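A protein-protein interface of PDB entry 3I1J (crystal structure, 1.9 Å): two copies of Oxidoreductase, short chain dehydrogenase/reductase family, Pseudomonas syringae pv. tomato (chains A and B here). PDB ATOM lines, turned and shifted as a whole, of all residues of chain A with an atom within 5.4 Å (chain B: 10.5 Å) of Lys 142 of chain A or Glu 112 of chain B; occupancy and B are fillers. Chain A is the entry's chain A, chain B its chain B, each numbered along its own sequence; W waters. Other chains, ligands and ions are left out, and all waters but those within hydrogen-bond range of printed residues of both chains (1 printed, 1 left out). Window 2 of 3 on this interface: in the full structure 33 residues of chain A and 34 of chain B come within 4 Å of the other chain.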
ATOM      1  N   LEU A  95     -10.921   8.693  15.937  1.00  0.00           N
ATOM      2  CA  LEU A  95      -9.905   9.701  16.207  1.00  0.00           C
ATOM      3  C   LEU A  95      -9.093   9.869  14.931  1.00  0.00           C
ATOM      4  O   LEU A  95      -8.663   8.886  14.351  1.00  0.00           O
ATOM      5  CB  LEU A  95      -9.002   9.248  17.366  1.00  0.00           C
ATOM      6  CG  LEU A  95      -8.065  10.272  18.019  1.00  0.00           C
ATOM      7  CD1 LEU A  95      -8.817  11.479  18.639  1.00  0.00           C
ATOM      8  CD2 LEU A  95      -7.241   9.576  19.127  1.00  0.00           C
ATOM      9  N   ARG A 135      -2.079   2.192  22.436  1.00  0.00           N
ATOM     10  CA  ARG A 135      -2.826   0.961  22.361  1.00  0.00           C
ATOM     11  C   ARG A 135      -4.340   1.118  22.606  1.00  0.00           C
ATOM     12  O   ARG A 135      -5.132   0.524  21.888  1.00  0.00           O
ATOM     13  CB  ARG A 135      -2.221  -0.082  23.297  1.00  0.00           C
ATOM     14  CG  ARG A 135      -2.495  -1.474  22.849  1.00  0.00           C
ATOM     15  CD  ARG A 135      -1.694  -2.466  23.647  1.00  0.00           C
ATOM     16  NE  ARG A 135      -2.376  -2.870  24.868  1.00  0.00           N
ATOM     17  CZ  ARG A 135      -3.185  -3.928  24.941  1.00  0.00           C
ATOM     18  NH1 ARG A 135      -3.771  -4.233  26.086  1.00  0.00           N
ATOM     19  NH2 ARG A 135      -3.418  -4.671  23.868  1.00  0.00           N
ATOM     20  N   LEU A 137      -6.153   3.829  22.024  1.00  0.00           N
ATOM     21  CA  LEU A 137      -6.702   4.676  20.964  1.00  0.00           C
ATOM     22  C   LEU A 137      -6.534   4.188  19.545  1.00  0.00           C
ATOM     23  O   LEU A 137      -7.222   4.662  18.640  1.00  0.00           O
ATOM     24  CB  LEU A 137      -6.166   6.095  21.068  1.00  0.00           C
ATOM     25  CG  LEU A 137      -6.530   6.825  22.362  1.00  0.00           C
ATOM     26  CD1 LEU A 137      -5.643   8.131  22.384  1.00  0.00           C
ATOM     27  CD2 LEU A 137      -8.068   7.113  22.485  1.00  0.00           C
ATOM     28  N   LEU A 138      -5.632   3.235  19.338  1.00  0.00           N
ATOM     29  CA  LEU A 138      -5.449   2.664  17.990  1.00  0.00           C
ATOM     30  C   LEU A 138      -6.779   2.198  17.328  1.00  0.00           C
ATOM     31  O   LEU A 138      -7.006   2.508  16.158  1.00  0.00           O
ATOM     32  CB  LEU A 138      -4.409   1.539  18.008  1.00  0.00           C
ATOM     33  CG  LEU A 138      -2.963   1.968  17.761  1.00  0.00           C
ATOM     34  CD1 LEU A 138      -1.948   0.832  18.106  1.00  0.00           C
ATOM     35  CD2 LEU A 138      -2.837   2.352  16.260  1.00  0.00           C
ATOM     36  N   PRO A 139      -7.649   1.451  18.043  1.00  0.00           N
ATOM     37  CA  PRO A 139      -8.912   1.087  17.321  1.00  0.00           C
ATOM     38  C   PRO A 139      -9.726   2.296  16.785  1.00  0.00           C
ATOM     39  O   PRO A 139     -10.224   2.250  15.665  1.00  0.00           O
ATOM     40  CB  PRO A 139      -9.713   0.300  18.362  1.00  0.00           C
ATOM     41  CG  PRO A 139      -8.599  -0.270  19.337  1.00  0.00           C
ATOM     42  CD  PRO A 139      -7.600   0.873  19.408  1.00  0.00           C
ATOM     43  N   LEU A 140      -9.817   3.371  17.577  1.00  0.00           N
ATOM     44  CA  LEU A 140     -10.415   4.647  17.128  1.00  0.00           C
ATOM     45  C   LEU A 140      -9.695   5.304  15.943  1.00  0.00           C
ATOM     46  O   LEU A 140     -10.331   5.788  14.979  1.00  0.00           O
ATOM     47  CB  LEU A 140     -10.454   5.636  18.302  1.00  0.00           C
ATOM     48  CG  LEU A 140     -11.564   5.398  19.336  1.00  0.00           C
ATOM     49  CD1 LEU A 140     -11.304   6.132  20.628  1.00  0.00           C
ATOM     50  CD2 LEU A 140     -12.885   5.830  18.775  1.00  0.00           C
ATOM     51  N   LEU A 141      -8.366   5.338  16.018  1.00  0.00           N
ATOM     52  CA  LEU A 141      -7.542   5.881  14.912  1.00  0.00           C
ATOM     53  C   LEU A 141      -7.766   5.062  13.633  1.00  0.00           C
ATOM     54  O   LEU A 141      -7.782   5.585  12.534  1.00  0.00           O
ATOM     55  CB  LEU A 141      -6.062   5.892  15.314  1.00  0.00           C
ATOM     56  CG  LEU A 141      -5.712   6.936  16.406  1.00  0.00           C
ATOM     57  CD1 LEU A 141      -4.479   6.499  17.242  1.00  0.00           C
ATOM     58  CD2 LEU A 141      -5.503   8.299  15.774  1.00  0.00           C
ATOM     59  N   LYS A 142      -7.964   3.770  13.803  1.00  0.00           N
ATOM     60  CA  LYS A 142      -8.204   2.885  12.664  1.00  0.00           C
ATOM     61  C   LYS A 142      -9.591   3.062  12.030  1.00  0.00           C
ATOM     62  O   LYS A 142      -9.836   2.569  10.914  1.00  0.00           O
ATOM     63  CB  LYS A 142      -7.889   1.431  13.037  1.00  0.00           C
ATOM     64  CG  LYS A 142      -6.391   1.125  13.084  1.00  0.00           C
ATOM     65  CD  LYS A 142      -6.072  -0.090  13.984  1.00  0.00           C
ATOM     66  CE  LYS A 142      -6.568  -1.391  13.420  1.00  0.00           C
ATOM     67  NZ  LYS A 142      -5.607  -1.891  12.384  1.00  0.00           N
ATOM     68  N   ARG A 143     -10.496   3.781  12.701  1.00  0.00           N
ATOM     69  CA  ARG A 143     -11.823   4.064  12.112  1.00  0.00           C
ATOM     70  C   ARG A 143     -11.807   5.334  11.255  1.00  0.00           C
ATOM     71  O   ARG A 143     -12.751   5.611  10.513  1.00  0.00           O
ATOM     72  CB  ARG A 143     -12.906   4.181  13.193  1.00  0.00           C
ATOM     73  CG  ARG A 143     -13.063   2.971  14.101  1.00  0.00           C
ATOM     74  CD  ARG A 143     -13.601   1.751  13.364  1.00  0.00           C
ATOM     75  NE  ARG A 143     -14.786   2.099  12.576  1.00  0.00           N
ATOM     76  CZ  ARG A 143     -15.449   1.254  11.794  1.00  0.00           C
ATOM     77  NH1 ARG A 143     -16.507   1.689  11.119  1.00  0.00           N
ATOM     78  NH2 ARG A 143     -15.068  -0.018  11.688  1.00  0.00           N
ATOM     79  N   SER A 144     -10.725   6.105  11.379  1.00  0.00           N
ATOM     80  CA  SER A 144     -10.462   7.264  10.520  1.00  0.00           C
ATOM     81  C   SER A 144     -10.172   6.913   9.046  1.00  0.00           C
ATOM     82  O   SER A 144      -9.554   5.905   8.738  1.00  0.00           O
ATOM     83  CB  SER A 144      -9.289   8.060  11.109  1.00  0.00           C
ATOM     84  OG  SER A 144      -8.962   9.226  10.365  1.00  0.00           O
ATOM     85  N   ALA A 147      -5.562   8.984   9.402  1.00  0.00           N
ATOM     86  CA  ALA A 147      -5.209   9.264  10.797  1.00  0.00           C
ATOM     87  C   ALA A 147      -3.704   9.421  10.979  1.00  0.00           C
ATOM     88  O   ALA A 147      -2.895   8.860  10.195  1.00  0.00           O
ATOM     89  CB  ALA A 147      -5.772   8.193  11.735  1.00  0.00           C
ATOM     90  N   GLU A 184       4.213  -1.536  11.450  1.00  0.00           N
ATOM     91  CA  GLU A 184       2.979  -2.312  11.559  1.00  0.00           C
ATOM     92  C   GLU A 184       1.786  -1.643  10.857  1.00  0.00           C
ATOM     93  O   GLU A 184       0.927  -2.330  10.298  1.00  0.00           O
ATOM     94  CB  GLU A 184       2.669  -2.626  13.033  1.00  0.00           C
ATOM     95  CG  GLU A 184       3.765  -3.430  13.708  1.00  0.00           C
ATOM     96  CD  GLU A 184       3.608  -3.560  15.204  1.00  0.00           C
ATOM     97  OE1 GLU A 184       2.628  -2.998  15.781  1.00  0.00           O
ATOM     98  OE2 GLU A 184       4.488  -4.223  15.797  1.00  0.00           O
ATOM     99  N   LEU A 185       1.751  -0.315  10.833  1.00  0.00           N
ATOM    100  CA  LEU A 185       0.615   0.410  10.235  1.00  0.00           C
ATOM    101  C   LEU A 185       0.668   0.526   8.720  1.00  0.00           C
ATOM    102  O   LEU A 185      -0.354   0.757   8.083  1.00  0.00           O
ATOM    103  CB  LEU A 185       0.551   1.829  10.800  1.00  0.00           C
ATOM    104  CG  LEU A 185       0.280   1.964  12.295  1.00  0.00           C
ATOM    105  CD1 LEU A 185       0.478   3.413  12.680  1.00  0.00           C
ATOM    106  CD2 LEU A 185      -1.113   1.427  12.654  1.00  0.00           C
ATOM    107  N   VAL A 188      -1.506  -1.437   5.549  1.00  0.00           N
ATOM    108  CA  VAL A 188      -2.637  -2.242   6.002  1.00  0.00           C
ATOM    109  C   VAL A 188      -3.659  -1.414   6.816  1.00  0.00           C
ATOM    110  O   VAL A 188      -4.738  -1.911   7.203  1.00  0.00           O
ATOM    111  CB  VAL A 188      -2.128  -3.505   6.751  1.00  0.00           C
ATOM    112  CG1 VAL A 188      -1.501  -4.467   5.754  1.00  0.00           C
ATOM    113  CG2 VAL A 188      -1.105  -3.135   7.856  1.00  0.00           C
ATOM    114  N   THR A 189      -3.305  -0.147   7.061  1.00  0.00           N
ATOM    115  CA  THR A 189      -4.179   0.824   7.731  1.00  0.00           C
ATOM    116  C   THR A 189      -4.068   2.202   7.074  1.00  0.00           C
ATOM    117  O   THR A 189      -3.220   2.419   6.204  1.00  0.00           O
ATOM    118  CB  THR A 189      -3.827   1.016   9.245  1.00  0.00           C
ATOM    119  OG1 THR A 189      -2.700   1.896   9.382  1.00  0.00           O
ATOM    120  CG2 THR A 189      -3.520  -0.309   9.924  1.00  0.00           C
ATOM    121  N   VAL A 191      -3.439   4.838   9.012  1.00  0.00           N
ATOM    122  CA  VAL A 191      -2.818   5.571  10.105  1.00  0.00           C
ATOM    123  C   VAL A 191      -1.328   5.662   9.829  1.00  0.00           C
ATOM    124  O   VAL A 191      -0.688   4.650   9.519  1.00  0.00           O
ATOM    125  CB  VAL A 191      -3.018   4.884  11.483  1.00  0.00           C
ATOM    126  CG1 VAL A 191      -2.604   5.797  12.627  1.00  0.00           C
ATOM    127  CG2 VAL A 191      -4.499   4.411  11.672  1.00  0.00           C
ATOM    128  N   PRO B 107       6.187 -11.148  24.247  1.00  0.00           N
ATOM    129  CA  PRO B 107       5.408 -11.572  23.077  1.00  0.00           C
ATOM    130  C   PRO B 107       5.846 -10.888  21.755  1.00  0.00           C
ATOM    131  O   PRO B 107       6.226  -9.699  21.729  1.00  0.00           O
ATOM    132  CB  PRO B 107       3.952 -11.224  23.446  1.00  0.00           C
ATOM    133  CG  PRO B 107       3.952 -11.012  24.974  1.00  0.00           C
ATOM    134  CD  PRO B 107       5.353 -10.542  25.309  1.00  0.00           C
ATOM    135  N   ARG B 108       5.815 -11.672  20.679  1.00  0.00           N
ATOM    136  CA  ARG B 108       6.028 -11.176  19.325  1.00  0.00           C
ATOM    137  C   ARG B 108       4.659 -11.030  18.673  1.00  0.00           C
ATOM    138  O   ARG B 108       4.181 -11.916  17.970  1.00  0.00           O
ATOM    139  CB  ARG B 108       6.914 -12.165  18.550  1.00  0.00           C
ATOM    140  CG  ARG B 108       8.371 -12.152  18.998  1.00  0.00           C
ATOM    141  CD  ARG B 108       9.280 -11.418  18.003  1.00  0.00           C
ATOM    142  NE  ARG B 108       9.947 -12.374  17.096  1.00  0.00           N
ATOM    143  CZ  ARG B 108       9.926 -12.301  15.762  1.00  0.00           C
ATOM    144  NH1 ARG B 108       9.295 -11.305  15.142  1.00  0.00           N
ATOM    145  NH2 ARG B 108      10.546 -13.227  15.033  1.00  0.00           N
ATOM    146  N   THR B 109       3.992  -9.929  18.979  1.00  0.00           N
ATOM    147  CA  THR B 109       2.647  -9.662  18.488  1.00  0.00           C
ATOM    148  C   THR B 109       2.748  -8.211  18.053  1.00  0.00           C
ATOM    149  O   THR B 109       3.673  -7.526  18.523  1.00  0.00           O
ATOM    150  CB  THR B 109       1.596  -9.783  19.626  1.00  0.00           C
ATOM    151  OG1 THR B 109       1.844  -8.766  20.619  1.00  0.00           O
ATOM    152  CG2 THR B 109       1.706 -11.108  20.303  1.00  0.00           C
ATOM    153  N   PRO B 110       1.835  -7.735  17.164  1.00  0.00           N
ATOM    154  CA  PRO B 110       1.753  -6.290  16.881  1.00  0.00           C
ATOM    155  C   PRO B 110       1.492  -5.515  18.172  1.00  0.00           C
ATOM    156  O   PRO B 110       0.926  -6.076  19.120  1.00  0.00           O
ATOM    157  CB  PRO B 110       0.559  -6.160  15.952  1.00  0.00           C
ATOM    158  CG  PRO B 110       0.311  -7.516  15.403  1.00  0.00           C
ATOM    159  CD  PRO B 110       0.864  -8.516  16.374  1.00  0.00           C
ATOM    160  N   LEU B 111       1.939  -4.253  18.216  1.00  0.00           N
ATOM    161  CA  LEU B 111       1.792  -3.392  19.409  1.00  0.00           C
ATOM    162  C   LEU B 111       0.342  -3.281  19.879  1.00  0.00           C
ATOM    163  O   LEU B 111       0.091  -3.287  21.080  1.00  0.00           O
ATOM    164  CB  LEU B 111       2.387  -1.989  19.149  1.00  0.00           C
ATOM    165  CG  LEU B 111       3.891  -1.960  18.805  1.00  0.00           C
ATOM    166  CD1 LEU B 111       4.314  -0.606  18.280  1.00  0.00           C
ATOM    167  CD2 LEU B 111       4.730  -2.284  20.042  1.00  0.00           C
ATOM    168  N   GLU B 112      -0.594  -3.221  18.927  1.00  0.00           N
ATOM    169  CA  GLU B 112      -2.027  -3.124  19.217  1.00  0.00           C
ATOM    170  C   GLU B 112      -2.541  -4.296  20.055  1.00  0.00           C
ATOM    171  O   GLU B 112      -3.531  -4.145  20.771  1.00  0.00           O
ATOM    172  CB  GLU B 112      -2.867  -2.971  17.933  1.00  0.00           C
ATOM    173  CG  GLU B 112      -3.093  -4.265  17.122  1.00  0.00           C
ATOM    174  CD  GLU B 112      -4.070  -4.122  15.942  1.00  0.00           C
ATOM    175  OE1 GLU B 112      -4.882  -3.164  15.894  1.00  0.00           O
ATOM    176  OE2 GLU B 112      -4.036  -5.001  15.053  1.00  0.00           O
ATOM    177  N   GLN B 113      -1.864  -5.444  19.954  1.00  0.00           N
ATOM    178  CA  GLN B 113      -2.233  -6.664  20.677  1.00  0.00           C
ATOM    179  C   GLN B 113      -1.308  -7.029  21.837  1.00  0.00           C
ATOM    180  O   GLN B 113      -1.496  -8.072  22.461  1.00  0.00           O
ATOM    181  CB  GLN B 113      -2.298  -7.874  19.724  1.00  0.00           C
ATOM    182  CG  GLN B 113      -3.271  -7.759  18.556  1.00  0.00           C
ATOM    183  CD  GLN B 113      -3.159  -8.951  17.613  1.00  0.00           C
ATOM    184  OE1 GLN B 113      -2.595 -10.000  17.969  1.00  0.00           O
ATOM    185  NE2 GLN B 113      -3.686  -8.796  16.403  1.00  0.00           N
ATOM    186  N   LEU B 114      -0.290  -6.220  22.104  1.00  0.00           N
ATOM    187  CA  LEU B 114       0.686  -6.576  23.125  1.00  0.00           C
ATOM    188  C   LEU B 114       0.125  -6.131  24.467  1.00  0.00           C
ATOM    189  O   LEU B 114      -0.151  -4.951  24.625  1.00  0.00           O
ATOM    190  CB  LEU B 114       2.022  -5.884  22.855  1.00  0.00           C
ATOM    191  CG  LEU B 114       3.126  -6.018  23.899  1.00  0.00           C
ATOM    192  CD1 LEU B 114       3.607  -7.455  24.010  1.00  0.00           C
ATOM    193  CD2 LEU B 114       4.292  -5.099  23.595  1.00  0.00           C
ATOM    194  N   PRO B 115      -0.107  -7.073  25.412  1.00  0.00           N
ATOM    195  CA  PRO B 115      -0.644  -6.627  26.713  1.00  0.00           C
ATOM    196  C   PRO B 115       0.191  -5.567  27.398  1.00  0.00           C
ATOM    197  O   PRO B 115       1.420  -5.623  27.353  1.00  0.00           O
ATOM    198  CB  PRO B 115      -0.605  -7.898  27.560  1.00  0.00           C
ATOM    199  CG  PRO B 115      -0.852  -9.005  26.547  1.00  0.00           C
ATOM    200  CD  PRO B 115       0.038  -8.542  25.365  1.00  0.00           C
ATOM    201  N   ASP B 116      -0.465  -4.621  28.070  1.00  0.00           N
ATOM    202  CA  ASP B 116       0.296  -3.555  28.783  1.00  0.00           C
ATOM    203  C   ASP B 116       1.324  -4.128  29.746  1.00  0.00           C
ATOM    204  O   ASP B 116       2.448  -3.597  29.883  1.00  0.00           O
ATOM    205  CB  ASP B 116      -0.650  -2.683  29.588  1.00  0.00           C
ATOM    206  CG  ASP B 116      -1.722  -2.062  28.741  1.00  0.00           C
ATOM    207  OD1 ASP B 116      -1.531  -1.892  27.526  1.00  0.00           O
ATOM    208  OD2 ASP B 116      -2.738  -1.661  29.312  1.00  0.00           O
ATOM    209  N   PHE B 119       4.491  -5.353  27.946  1.00  0.00           N
ATOM    210  CA  PHE B 119       5.329  -4.212  27.489  1.00  0.00           C
ATOM    211  C   PHE B 119       6.117  -3.682  28.687  1.00  0.00           C
ATOM    212  O   PHE B 119       7.341  -3.539  28.606  1.00  0.00           O
ATOM    213  CB  PHE B 119       4.474  -3.111  26.838  1.00  0.00           C
ATOM    214  CG  PHE B 119       5.270  -1.926  26.363  1.00  0.00           C
ATOM    215  CD1 PHE B 119       5.650  -1.820  25.025  1.00  0.00           C
ATOM    216  CD2 PHE B 119       5.656  -0.919  27.257  1.00  0.00           C
ATOM    217  CE1 PHE B 119       6.422  -0.720  24.574  1.00  0.00           C
ATOM    218  CE2 PHE B 119       6.425   0.184  26.808  1.00  0.00           C
ATOM    219  CZ  PHE B 119       6.802   0.265  25.474  1.00  0.00           C
ATOM    220  N   ALA B 162       8.239  -4.437  12.557  1.00  0.00           N
ATOM    221  CA  ALA B 162       6.940  -4.955  13.002  1.00  0.00           C
ATOM    222  C   ALA B 162       7.043  -6.250  13.809  1.00  0.00           C
ATOM    223  O   ALA B 162       7.887  -7.133  13.541  1.00  0.00           O
ATOM    224  CB  ALA B 162       6.012  -5.167  11.806  1.00  0.00           C
ATOM    225  N   ASN B 163       6.160  -6.324  14.800  1.00  0.00           N
ATOM    226  CA  ASN B 163       5.943  -7.494  15.682  1.00  0.00           C
ATOM    227  C   ASN B 163       7.100  -7.887  16.588  1.00  0.00           C
ATOM    228  O   ASN B 163       7.196  -9.034  17.023  1.00  0.00           O
ATOM    229  CB  ASN B 163       5.437  -8.702  14.902  1.00  0.00           C
ATOM    230  CG  ASN B 163       4.125  -8.428  14.187  1.00  0.00           C
ATOM    231  OD1 ASN B 163       3.614  -7.307  14.183  1.00  0.00           O
ATOM    232  ND2 ASN B 163       3.572  -9.456  13.583  1.00  0.00           N
ATOM    233  N   TRP B 164       7.990  -6.946  16.853  1.00  0.00           N
ATOM    234  CA  TRP B 164       9.046  -7.181  17.827  1.00  0.00           C
ATOM    235  C   TRP B 164       8.639  -6.658  19.214  1.00  0.00           C
ATOM    236  O   TRP B 164       9.430  -6.680  20.155  1.00  0.00           O
ATOM    237  CB  TRP B 164      10.378  -6.625  17.313  1.00  0.00           C
ATOM    238  CG  TRP B 164      11.047  -7.618  16.347  1.00  0.00           C
ATOM    239  CD1 TRP B 164      11.025  -7.601  14.971  1.00  0.00           C
ATOM    240  CD2 TRP B 164      11.777  -8.788  16.723  1.00  0.00           C
ATOM    241  NE1 TRP B 164      11.705  -8.703  14.475  1.00  0.00           N
ATOM    242  CE2 TRP B 164      12.193  -9.431  15.529  1.00  0.00           C
ATOM    243  CE3 TRP B 164      12.136  -9.351  17.959  1.00  0.00           C
ATOM    244  CZ2 TRP B 164      12.949 -10.607  15.538  1.00  0.00           C
ATOM    245  CZ3 TRP B 164      12.897 -10.533  17.960  1.00  0.00           C
ATOM    246  CH2 TRP B 164      13.289 -11.138  16.758  1.00  0.00           C
ATOM    247  N   GLY B 165       7.382  -6.211  19.323  1.00  0.00           N
ATOM    248  CA  GLY B 165       6.778  -5.784  20.609  1.00  0.00           C
ATOM    249  C   GLY B 165       7.596  -4.794  21.407  1.00  0.00           C
ATOM    250  O   GLY B 165       8.033  -3.754  20.886  1.00  0.00           O
ATOM    251  N   ALA B 166       7.808  -5.103  22.685  1.00  0.00           N
ATOM    252  CA  ALA B 166       8.640  -4.234  23.499  1.00  0.00           C
ATOM    253  C   ALA B 166      10.131  -4.509  23.303  1.00  0.00           C
ATOM    254  O   ALA B 166      10.965  -3.702  23.743  1.00  0.00           O
ATOM    255  CB  ALA B 166       8.256  -4.321  24.973  1.00  0.00           C
HETATM  256  O   HOH W   1       0.119  -2.560  16.067  1.00  0.00           O
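The backbone carbonyl oxygen of Glu 112 of chain B lies within hydrogen-bond range of the guanidinium group of Arg 135 of chain A (3.1 Å). The guanidinium group (NE) of Arg 135 of chain A lies within hydrogen-bond range of the backbone carbonyl oxygen (O) of Leu 114 of chain B (3.1 Å). NE of Arg 135 of chain A is in salt-bridge range of OD1 of Asp 116 of chain B (3.0 Å). OE1 of Glu 112 of chain B is in salt-bridge range of NZ of Lys 142 of chain A (3.8 Å). OE1 of Glu 184 of chain A is in hydrogen-bond range of N of Leu 111 of chain B, 2.8 Å away. N of Asn 163 of chain B sits at hydrogen-bond distance from OE2 of Glu 184 of chain A.
Water W1 lies within hydrogen-bond range of OE1 of Glu 184 of chain A, N of Glu 112 of chain B and N of Leu 111 of chain B.
No position is printed for both chains.
Among the printed residues, pairs that only touch across the chains: Arg 135 of chain A with Leu 111 of chain B (3.2 Å), Arg 135 of chain A with Gln 113 of chain B (3.8 Å), Arg 135 of chain A with Pro 115 of chain B (3.99 Å), Leu 138 of chain A with Glu 112 of chain B (3.9 Å), Glu 184 of chain A with Pro 110 of chain B (3.6 Å) and Glu 184 of chain A with Ala 162 of chain B (3.4 Å).
Of the 16 printed residues of chain A, 4 touch a printed residue of chain B. Printed residues of chain B that touch a printed residue of chain A: Pro 110, Leu 111, Glu 112, Gln 113, Leu 114, Pro 115, Asp 116, Ala 162 and Asn 163. Hydrophobic or aromatic side chains of chain B that line the printed part of chain A: Pro 110, Leu 111 and Ala 162.
Printed residues of chain B within 4 Å of Lys 142 of chain A: Glu 112. No residue of chain B comes within 4 Å of Ser 144 of chain A. Printed residues of chain A within 4 Å of Glu 112 of chain B: Arg 135 (3.1 Å), Leu 138 (3.9 Å) and Lys 142 (3.5 Å). Of the printed residues of chain A, Gln 113 of chain B touches Arg 135. Of the printed residues of chain A, Leu 114 of chain B touches Arg 135 (3.1 Å). Of the printed residues of chain A, Asn 163 of chain B touches Glu 184. The nearest printed residue of chain B that does not touch Lys 142 of chain A is Gln 113 of chain B (8.2 Å). The nearest printed residue of chain A that does not touch Glu 112 of chain B is Glu 184 of chain A (4.5 Å). The nearest printed residue of chain A that does not touch Asn 163 of chain B is Leu 185 of chain A (8.0 Å).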
